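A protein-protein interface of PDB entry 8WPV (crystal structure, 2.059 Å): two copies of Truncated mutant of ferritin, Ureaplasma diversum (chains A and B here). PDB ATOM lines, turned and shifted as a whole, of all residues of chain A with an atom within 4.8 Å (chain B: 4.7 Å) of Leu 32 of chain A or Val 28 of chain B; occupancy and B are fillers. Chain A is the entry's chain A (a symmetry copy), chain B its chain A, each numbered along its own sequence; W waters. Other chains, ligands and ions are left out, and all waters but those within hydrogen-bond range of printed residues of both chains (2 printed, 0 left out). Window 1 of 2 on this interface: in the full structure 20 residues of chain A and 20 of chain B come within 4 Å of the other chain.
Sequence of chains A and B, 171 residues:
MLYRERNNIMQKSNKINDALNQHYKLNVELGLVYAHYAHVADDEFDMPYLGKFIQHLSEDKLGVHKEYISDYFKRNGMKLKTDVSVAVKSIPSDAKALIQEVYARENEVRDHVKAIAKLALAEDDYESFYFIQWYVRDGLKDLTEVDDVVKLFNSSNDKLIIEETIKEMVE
The backbone carbonyl oxygen of Val 86 of chain A sits at hydrogen-bond distance from the backbone NH of Val 84 of chain B (2.7 Å).
Among the printed residues, merely in contact across the chains: His 36 of chain A with Thr 82 of chain B (2.8 Å), Leu 32 of chain A with Val 28 of chain B (3.6 Å), Val 28 of chain A with Leu 32 of chain B (3.6 Å) and Val 84 of chain A with Val 84 of chain B (3.9 Å).
Of the printed residues of chain B, Val 28 of chain A touches Leu 32. Of the printed residues of chain B, His 36 of chain A touches Thr 82 (2.8 Å). Of the printed residues of chain B, Val 84 of chain A touches Val 84. Val 28 of chain B touches just one residue of chain A: Leu 32. Of the printed residues of chain A, Thr 82 of chain B touches His 36. Of the printed residues of chain A, Val 84 of chain B touches Val 84 (3.9 Å) and Val 86 (2.7 Å). The nearest printed residue of chain A that does not touch Val 28 of chain B is Val 84 of chain A (6.5 Å). The nearest printed residue of chain B that does not touch Val 86 of chain A is Thr 82 of chain B (4.1 Å).
Printed residues of chain B that touch a printed residue of chain A: Val 28, Leu 32, Thr 82 and Val 84. Hydrophobic or aromatic side chains of chain B within 4 Å of the printed part of chain A: Val 28, Leu 32 and Val 84. Printed residues of chain A that touch a printed residue of chain B: Val 28, Leu 32, His 36, Val 84 and Val 86. Hydrophobic or aromatic side chains of chain A that line the printed part of chain B: Val 28, Leu 32, His 36, Val 84 and Val 86. Among the printed residues, 5 pairs touch across the chains. Among the printed residues, no Asp or Glu carboxylate lies within 4 Å of a Lys or Arg side-chain nitrogen of the other chain.
Val 28 of chain A touches Leu 32 of chain B, and with the chains exchanged Leu 32 of chain A touches Val 28 of chain B. Val 84 of chain A touches its own counterpart, Val 84 of chain B. Of the 5 pairs that touch across the chains among the printed residues, 3 have their exchanged pair printed and touching as well.
Water W2 lies within hydrogen-bond range of the side-chain hydroxyl (OG) of Ser 58 of chain A (2.6 Å) and the side-chain amino group (NZ) of Lys 66 of chain B (3.0 Å). Water W1 lies within hydrogen-bond range of OH of Tyr 24 of chain B (2.7 Å), OG1 of Thr 82 of chain B (2.7 Å) and O of Leu 32 of chain A (2.8 Å).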
ATOM      1  N   VAL A  28      15.452 -11.947 -21.639  1.00  0.00           N
ATOM      2  CA  VAL A  28      15.360 -11.249 -20.358  1.00  0.00           C
ATOM      3  C   VAL A  28      13.932 -10.781 -20.118  1.00  0.00           C
ATOM      4  O   VAL A  28      13.352 -11.009 -19.049  1.00  0.00           O
ATOM      5  CB  VAL A  28      16.353 -10.075 -20.314  1.00  0.00           C
ATOM      6  CG1 VAL A  28      16.041  -9.162 -19.140  1.00  0.00           C
ATOM      7  CG2 VAL A  28      17.778 -10.591 -20.231  1.00  0.00           C
ATOM      8  N   GLU A  29      13.339 -10.130 -21.118  1.00  0.00           N
ATOM      9  CA  GLU A  29      12.003  -9.572 -20.946  1.00  0.00           C
ATOM     10  C   GLU A  29      10.955 -10.671 -20.821  1.00  0.00           C
ATOM     11  O   GLU A  29      10.046 -10.573 -19.988  1.00  0.00           O
ATOM     12  CB  GLU A  29      11.692  -8.623 -22.104  1.00  0.00           C
ATOM     13  CG  GLU A  29      12.453  -7.308 -21.985  1.00  0.00           C
ATOM     14  CD  GLU A  29      12.381  -6.443 -23.229  1.00  0.00           C
ATOM     15  OE1 GLU A  29      13.009  -5.363 -23.227  1.00  0.00           O
ATOM     16  OE2 GLU A  29      11.710  -6.840 -24.206  1.00  0.00           O
ATOM     17  N   LEU A  30      11.071 -11.732 -21.625  1.00  0.00           N
ATOM     18  CA  LEU A  30      10.184 -12.880 -21.458  1.00  0.00           C
ATOM     19  C   LEU A  30      10.328 -13.491 -20.071  1.00  0.00           C
ATOM     20  O   LEU A  30       9.330 -13.855 -19.436  1.00  0.00           O
ATOM     21  CB  LEU A  30      10.467 -13.934 -22.529  1.00  0.00           C
ATOM     22  CG  LEU A  30       9.555 -13.956 -23.755  1.00  0.00           C
ATOM     23  CD1 LEU A  30       9.698 -15.278 -24.495  1.00  0.00           C
ATOM     24  CD2 LEU A  30       8.112 -13.723 -23.342  1.00  0.00           C
ATOM     25  N   GLY A  31      11.566 -13.613 -19.584  1.00  0.00           N
ATOM     26  CA  GLY A  31      11.779 -14.185 -18.263  1.00  0.00           C
ATOM     27  C   GLY A  31      11.107 -13.386 -17.164  1.00  0.00           C
ATOM     28  O   GLY A  31      10.556 -13.954 -16.218  1.00  0.00           O
ATOM     29  N   LEU A  32      11.133 -12.056 -17.279  1.00  0.00           N
ATOM     30  CA  LEU A  32      10.492 -11.219 -16.271  1.00  0.00           C
ATOM     31  C   LEU A  32       8.973 -11.319 -16.351  1.00  0.00           C
ATOM     32  O   LEU A  32       8.287 -11.253 -15.324  1.00  0.00           O
ATOM     33  CB  LEU A  32      10.951  -9.769 -16.426  1.00  0.00           C
ATOM     34  CG  LEU A  32      12.436  -9.556 -16.128  1.00  0.00           C
ATOM     35  CD1 LEU A  32      12.894  -8.164 -16.549  1.00  0.00           C
ATOM     36  CD2 LEU A  32      12.703  -9.796 -14.650  1.00  0.00           C
ATOM     37  N   VAL A  33       8.430 -11.479 -17.559  1.00  0.00           N
ATOM     38  CA  VAL A  33       6.987 -11.650 -17.702  1.00  0.00           C
ATOM     39  C   VAL A  33       6.548 -12.991 -17.123  1.00  0.00           C
ATOM     40  O   VAL A  33       5.539 -13.075 -16.411  1.00  0.00           O
ATOM     41  CB  VAL A  33       6.574 -11.506 -19.178  1.00  0.00           C
ATOM     42  CG1 VAL A  33       5.122 -11.916 -19.368  1.00  0.00           C
ATOM     43  CG2 VAL A  33       6.791 -10.081 -19.652  1.00  0.00           C
ATOM     44  N   TYR A  34       7.298 -14.057 -17.418  1.00  0.00           N
ATOM     45  CA  TYR A  34       6.939 -15.380 -16.916  1.00  0.00           C
ATOM     46  C   TYR A  34       6.978 -15.425 -15.393  1.00  0.00           C
ATOM     47  O   TYR A  34       6.136 -16.075 -14.763  1.00  0.00           O
ATOM     48  CB  TYR A  34       7.871 -16.441 -17.502  1.00  0.00           C
ATOM     49  CG  TYR A  34       7.646 -16.731 -18.969  1.00  0.00           C
ATOM     50  CD1 TYR A  34       6.567 -16.183 -19.653  1.00  0.00           C
ATOM     51  CD2 TYR A  34       8.512 -17.557 -19.671  1.00  0.00           C
ATOM     52  CE1 TYR A  34       6.362 -16.449 -20.995  1.00  0.00           C
ATOM     53  CE2 TYR A  34       8.318 -17.827 -21.009  1.00  0.00           C
ATOM     54  CZ  TYR A  34       7.242 -17.272 -21.667  1.00  0.00           C
ATOM     55  OH  TYR A  34       7.049 -17.546 -23.001  1.00  0.00           O
ATOM     56  N   ALA A  35       7.953 -14.743 -14.785  1.00  0.00           N
ATOM     57  CA  ALA A  35       8.013 -14.681 -13.328  1.00  0.00           C
ATOM     58  C   ALA A  35       6.738 -14.076 -12.757  1.00  0.00           C
ATOM     59  O   ALA A  35       6.223 -14.542 -11.733  1.00  0.00           O
ATOM     60  CB  ALA A  35       9.237 -13.880 -12.883  1.00  0.00           C
ATOM     61  N   HIS A  36       6.212 -13.041 -13.412  1.00  0.00           N
ATOM     62  CA  HIS A  36       4.933 -12.468 -13.004  1.00  0.00           C
ATOM     63  C   HIS A  36       3.795 -13.454 -13.234  1.00  0.00           C
ATOM     64  O   HIS A  36       2.953 -13.662 -12.351  1.00  0.00           O
ATOM     65  CB  HIS A  36       4.683 -11.167 -13.768  1.00  0.00           C
ATOM     66  CG  HIS A  36       3.720 -10.243 -13.092  1.00  0.00           C
ATOM     67  ND1 HIS A  36       2.362 -10.477 -13.061  1.00  0.00           N
ATOM     68  CD2 HIS A  36       3.916  -9.080 -12.430  1.00  0.00           C
ATOM     69  CE1 HIS A  36       1.765  -9.501 -12.401  1.00  0.00           C
ATOM     70  NE2 HIS A  36       2.685  -8.638 -12.011  1.00  0.00           N
ATOM     71  N   SER A  58      10.750 -19.234 -16.579  1.00  0.00           N
ATOM     72  CA  SER A  58      11.317 -17.921 -16.290  1.00  0.00           C
ATOM     73  C   SER A  58      12.807 -18.019 -15.986  1.00  0.00           C
ATOM     74  O   SER A  58      13.620 -17.290 -16.566  1.00  0.00           O
ATOM     75  CB  SER A  58      10.565 -17.284 -15.120  1.00  0.00           C
ATOM     76  OG  SER A  58      11.185 -16.081 -14.705  1.00  0.00           O
ATOM     77  N   LEU A  62      15.923 -16.359 -18.148  1.00  0.00           N
ATOM     78  CA  LEU A  62      16.821 -15.477 -17.414  1.00  0.00           C
ATOM     79  C   LEU A  62      18.128 -16.153 -17.024  1.00  0.00           C
ATOM     80  O   LEU A  62      19.014 -15.481 -16.486  1.00  0.00           O
ATOM     81  CB  LEU A  62      16.123 -14.950 -16.157  1.00  0.00           C
ATOM     82  CG  LEU A  62      15.132 -13.796 -16.328  1.00  0.00           C
ATOM     83  CD1 LEU A  62      14.303 -13.603 -15.062  1.00  0.00           C
ATOM     84  CD2 LEU A  62      15.854 -12.509 -16.701  1.00  0.00           C
ATOM     85  N   VAL A  84      16.733  -2.931 -21.539  1.00  0.00           N
ATOM     86  CA  VAL A  84      15.604  -3.745 -21.115  1.00  0.00           C
ATOM     87  C   VAL A  84      14.446  -2.837 -20.734  1.00  0.00           C
ATOM     88  O   VAL A  84      14.615  -1.894 -19.953  1.00  0.00           O
ATOM     89  CB  VAL A  84      15.978  -4.673 -19.944  1.00  0.00           C
ATOM     90  CG1 VAL A  84      14.732  -5.331 -19.366  1.00  0.00           C
ATOM     91  CG2 VAL A  84      16.966  -5.725 -20.418  1.00  0.00           C
ATOM     92  N   VAL A  86      10.271  -3.601 -19.877  1.00  0.00           N
ATOM     93  CA  VAL A  86       9.120  -4.491 -19.830  1.00  0.00           C
ATOM     94  C   VAL A  86       8.212  -4.067 -18.686  1.00  0.00           C
ATOM     95  O   VAL A  86       8.669  -3.769 -17.577  1.00  0.00           O
ATOM     96  CB  VAL A  86       9.547  -5.974 -19.712  1.00  0.00           C
ATOM     97  CG1 VAL A  86      10.097  -6.308 -18.328  1.00  0.00           C
ATOM     98  CG2 VAL A  86       8.388  -6.886 -20.074  1.00  0.00           C
ATOM     99  N   TYR B  24      11.651  -4.852  -5.298  1.00  0.00           N
ATOM    100  CA  TYR B  24      11.643  -5.884  -6.331  1.00  0.00           C
ATOM    101  C   TYR B  24      12.196  -5.337  -7.641  1.00  0.00           C
ATOM    102  O   TYR B  24      13.035  -5.969  -8.292  1.00  0.00           O
ATOM    103  CB  TYR B  24      10.215  -6.405  -6.513  1.00  0.00           C
ATOM    104  CG  TYR B  24      10.041  -7.509  -7.536  1.00  0.00           C
ATOM    105  CD1 TYR B  24       9.780  -7.215  -8.869  1.00  0.00           C
ATOM    106  CD2 TYR B  24      10.102  -8.844  -7.160  1.00  0.00           C
ATOM    107  CE1 TYR B  24       9.606  -8.220  -9.803  1.00  0.00           C
ATOM    108  CE2 TYR B  24       9.929  -9.855  -8.086  1.00  0.00           C
ATOM    109  CZ  TYR B  24       9.682  -9.537  -9.406  1.00  0.00           C
ATOM    110  OH  TYR B  24       9.510 -10.541 -10.330  1.00  0.00           O
ATOM    111  N   LYS B  25      11.737  -4.145  -8.029  1.00  0.00           N
ATOM    112  CA  LYS B  25      12.214  -3.502  -9.247  1.00  0.00           C
ATOM    113  C   LYS B  25      13.706  -3.197  -9.166  1.00  0.00           C
ATOM    114  O   LYS B  25      14.441  -3.389 -10.143  1.00  0.00           O
ATOM    115  CB  LYS B  25      11.400  -2.228  -9.482  1.00  0.00           C
ATOM    116  CG  LYS B  25      11.899  -1.284 -10.559  1.00  0.00           C
ATOM    117  CD  LYS B  25      10.998  -0.049 -10.595  1.00  0.00           C
ATOM    118  CE  LYS B  25      11.565   1.067 -11.454  1.00  0.00           C
ATOM    119  NZ  LYS B  25      11.400   0.792 -12.907  1.00  0.00           N
ATOM    120  N   LEU B  26      14.173  -2.739  -8.002  1.00  0.00           N
ATOM    121  CA  LEU B  26      15.590  -2.422  -7.841  1.00  0.00           C
ATOM    122  C   LEU B  26      16.457  -3.666  -7.982  1.00  0.00           C
ATOM    123  O   LEU B  26      17.502  -3.631  -8.642  1.00  0.00           O
ATOM    124  CB  LEU B  26      15.824  -1.757  -6.486  1.00  0.00           C
ATOM    125  CG  LEU B  26      17.274  -1.446  -6.114  1.00  0.00           C
ATOM    126  CD1 LEU B  26      17.868  -0.417  -7.065  1.00  0.00           C
ATOM    127  CD2 LEU B  26      17.358  -0.959  -4.674  1.00  0.00           C
ATOM    128  N   ASN B  27      16.039  -4.779  -7.375  1.00  0.00           N
ATOM    129  CA  ASN B  27      16.840  -5.997  -7.438  1.00  0.00           C
ATOM    130  C   ASN B  27      16.904  -6.552  -8.857  1.00  0.00           C
ATOM    131  O   ASN B  27      17.946  -7.064  -9.282  1.00  0.00           O
ATOM    132  CB  ASN B  27      16.282  -7.042  -6.474  1.00  0.00           C
ATOM    133  CG  ASN B  27      16.836  -6.887  -5.071  1.00  0.00           C
ATOM    134  OD1 ASN B  27      17.998  -7.201  -4.812  1.00  0.00           O
ATOM    135  ND2 ASN B  27      16.010  -6.393  -4.157  1.00  0.00           N
ATOM    136  N   VAL B  28      15.803  -6.461  -9.603  1.00  0.00           N
ATOM    137  CA  VAL B  28      15.807  -6.917 -10.991  1.00  0.00           C
ATOM    138  C   VAL B  28      16.757  -6.064 -11.819  1.00  0.00           C
ATOM    139  O   VAL B  28      17.606  -6.580 -12.557  1.00  0.00           O
ATOM    140  CB  VAL B  28      14.381  -6.894 -11.568  1.00  0.00           C
ATOM    141  CG1 VAL B  28      14.419  -7.050 -13.079  1.00  0.00           C
ATOM    142  CG2 VAL B  28      13.538  -7.986 -10.935  1.00  0.00           C
ATOM    143  N   GLU B  29      16.637  -4.742 -11.697  1.00  0.00           N
ATOM    144  CA  GLU B  29      17.447  -3.849 -12.516  1.00  0.00           C
ATOM    145  C   GLU B  29      18.918  -3.917 -12.121  1.00  0.00           C
ATOM    146  O   GLU B  29      19.797  -3.931 -12.992  1.00  0.00           O
ATOM    147  CB  GLU B  29      16.900  -2.425 -12.415  1.00  0.00           C
ATOM    148  CG  GLU B  29      15.601  -2.255 -13.195  1.00  0.00           C
ATOM    149  CD  GLU B  29      14.888  -0.946 -12.918  1.00  0.00           C
ATOM    150  OE1 GLU B  29      13.796  -0.744 -13.491  1.00  0.00           O
ATOM    151  OE2 GLU B  29      15.405  -0.126 -12.129  1.00  0.00           O
ATOM    152  N   LEU B  30      19.207  -3.977 -10.818  1.00  0.00           N
ATOM    153  CA  LEU B  30      20.585  -4.185 -10.381  1.00  0.00           C
ATOM    154  C   LEU B  30      21.138  -5.502 -10.910  1.00  0.00           C
ATOM    155  O   LEU B  30      22.291  -5.567 -11.354  1.00  0.00           O
ATOM    156  CB  LEU B  30      20.673  -4.154  -8.855  1.00  0.00           C
ATOM    157  CG  LEU B  30      21.119  -2.847  -8.200  1.00  0.00           C
ATOM    158  CD1 LEU B  30      21.545  -3.097  -6.762  1.00  0.00           C
ATOM    159  CD2 LEU B  30      22.251  -2.221  -8.997  1.00  0.00           C
ATOM    160  N   GLY B  31      20.329  -6.564 -10.870  1.00  0.00           N
ATOM    161  CA  GLY B  31      20.789  -7.853 -11.362  1.00  0.00           C
ATOM    162  C   GLY B  31      21.160  -7.820 -12.832  1.00  0.00           C
ATOM    163  O   GLY B  31      22.141  -8.440 -13.249  1.00  0.00           O
ATOM    164  N   LEU B  32      20.388  -7.087 -13.636  1.00  0.00           N
ATOM    165  CA  LEU B  32      20.691  -6.989 -15.059  1.00  0.00           C
ATOM    166  C   LEU B  32      21.946  -6.159 -15.304  1.00  0.00           C
ATOM    167  O   LEU B  32      22.709  -6.440 -16.235  1.00  0.00           O
ATOM    168  CB  LEU B  32      19.495  -6.404 -15.811  1.00  0.00           C
ATOM    169  CG  LEU B  32      18.259  -7.304 -15.802  1.00  0.00           C
ATOM    170  CD1 LEU B  32      17.031  -6.569 -16.328  1.00  0.00           C
ATOM    171  CD2 LEU B  32      18.534  -8.561 -16.614  1.00  0.00           C
ATOM    172  N   LEU B  62      18.673 -11.283  -8.982  1.00  0.00           N
ATOM    173  CA  LEU B  62      17.650 -11.819  -9.871  1.00  0.00           C
ATOM    174  C   LEU B  62      17.062 -13.133  -9.375  1.00  0.00           C
ATOM    175  O   LEU B  62      16.115 -13.636  -9.988  1.00  0.00           O
ATOM    176  CB  LEU B  62      18.228 -12.015 -11.275  1.00  0.00           C
ATOM    177  CG  LEU B  62      18.354 -10.778 -12.168  1.00  0.00           C
ATOM    178  CD1 LEU B  62      19.222 -11.078 -13.387  1.00  0.00           C
ATOM    179  CD2 LEU B  62      16.983 -10.271 -12.593  1.00  0.00           C
ATOM    180  N   LYS B  66      14.550 -11.274  -5.366  1.00  0.00           N
ATOM    181  CA  LYS B  66      13.272 -10.895  -5.949  1.00  0.00           C
ATOM    182  C   LYS B  66      12.171 -11.911  -5.670  1.00  0.00           C
ATOM    183  O   LYS B  66      11.002 -11.525  -5.552  1.00  0.00           O
ATOM    184  CB  LYS B  66      13.424 -10.675  -7.461  1.00  0.00           C
ATOM    185  CG  LYS B  66      13.137 -11.889  -8.337  1.00  0.00           C
ATOM    186  CD  LYS B  66      13.233 -11.519  -9.809  1.00  0.00           C
ATOM    187  CE  LYS B  66      12.651 -12.601 -10.705  1.00  0.00           C
ATOM    188  NZ  LYS B  66      13.297 -13.921 -10.463  1.00  0.00           N
ATOM    189  N   THR B  82       5.290  -5.649 -12.057  1.00  0.00           N
ATOM    190  CA  THR B  82       6.471  -5.806 -12.900  1.00  0.00           C
ATOM    191  C   THR B  82       6.555  -4.598 -13.824  1.00  0.00           C
ATOM    192  O   THR B  82       5.765  -4.467 -14.766  1.00  0.00           O
ATOM    193  CB  THR B  82       6.431  -7.108 -13.694  1.00  0.00           C
ATOM    194  OG1 THR B  82       6.593  -8.212 -12.797  1.00  0.00           O
ATOM    195  CG2 THR B  82       7.556  -7.136 -14.719  1.00  0.00           C
ATOM    196  N   VAL B  84       9.890  -2.675 -15.402  1.00  0.00           N
ATOM    197  CA  VAL B  84      11.343  -2.755 -15.429  1.00  0.00           C
ATOM    198  C   VAL B  84      11.871  -1.921 -16.584  1.00  0.00           C
ATOM    199  O   VAL B  84      11.411  -2.061 -17.723  1.00  0.00           O
ATOM    200  CB  VAL B  84      11.832  -4.211 -15.537  1.00  0.00           C
ATOM    201  CG1 VAL B  84      13.330  -4.252 -15.804  1.00  0.00           C
ATOM    202  CG2 VAL B  84      11.496  -4.962 -14.260  1.00  0.00           C
HETATM  203  O   HOH W   1       8.557 -10.080 -12.799  1.00  0.00           O
HETATM  204  O   HOH W   2      12.614 -15.945 -12.506  1.00  0.00           O
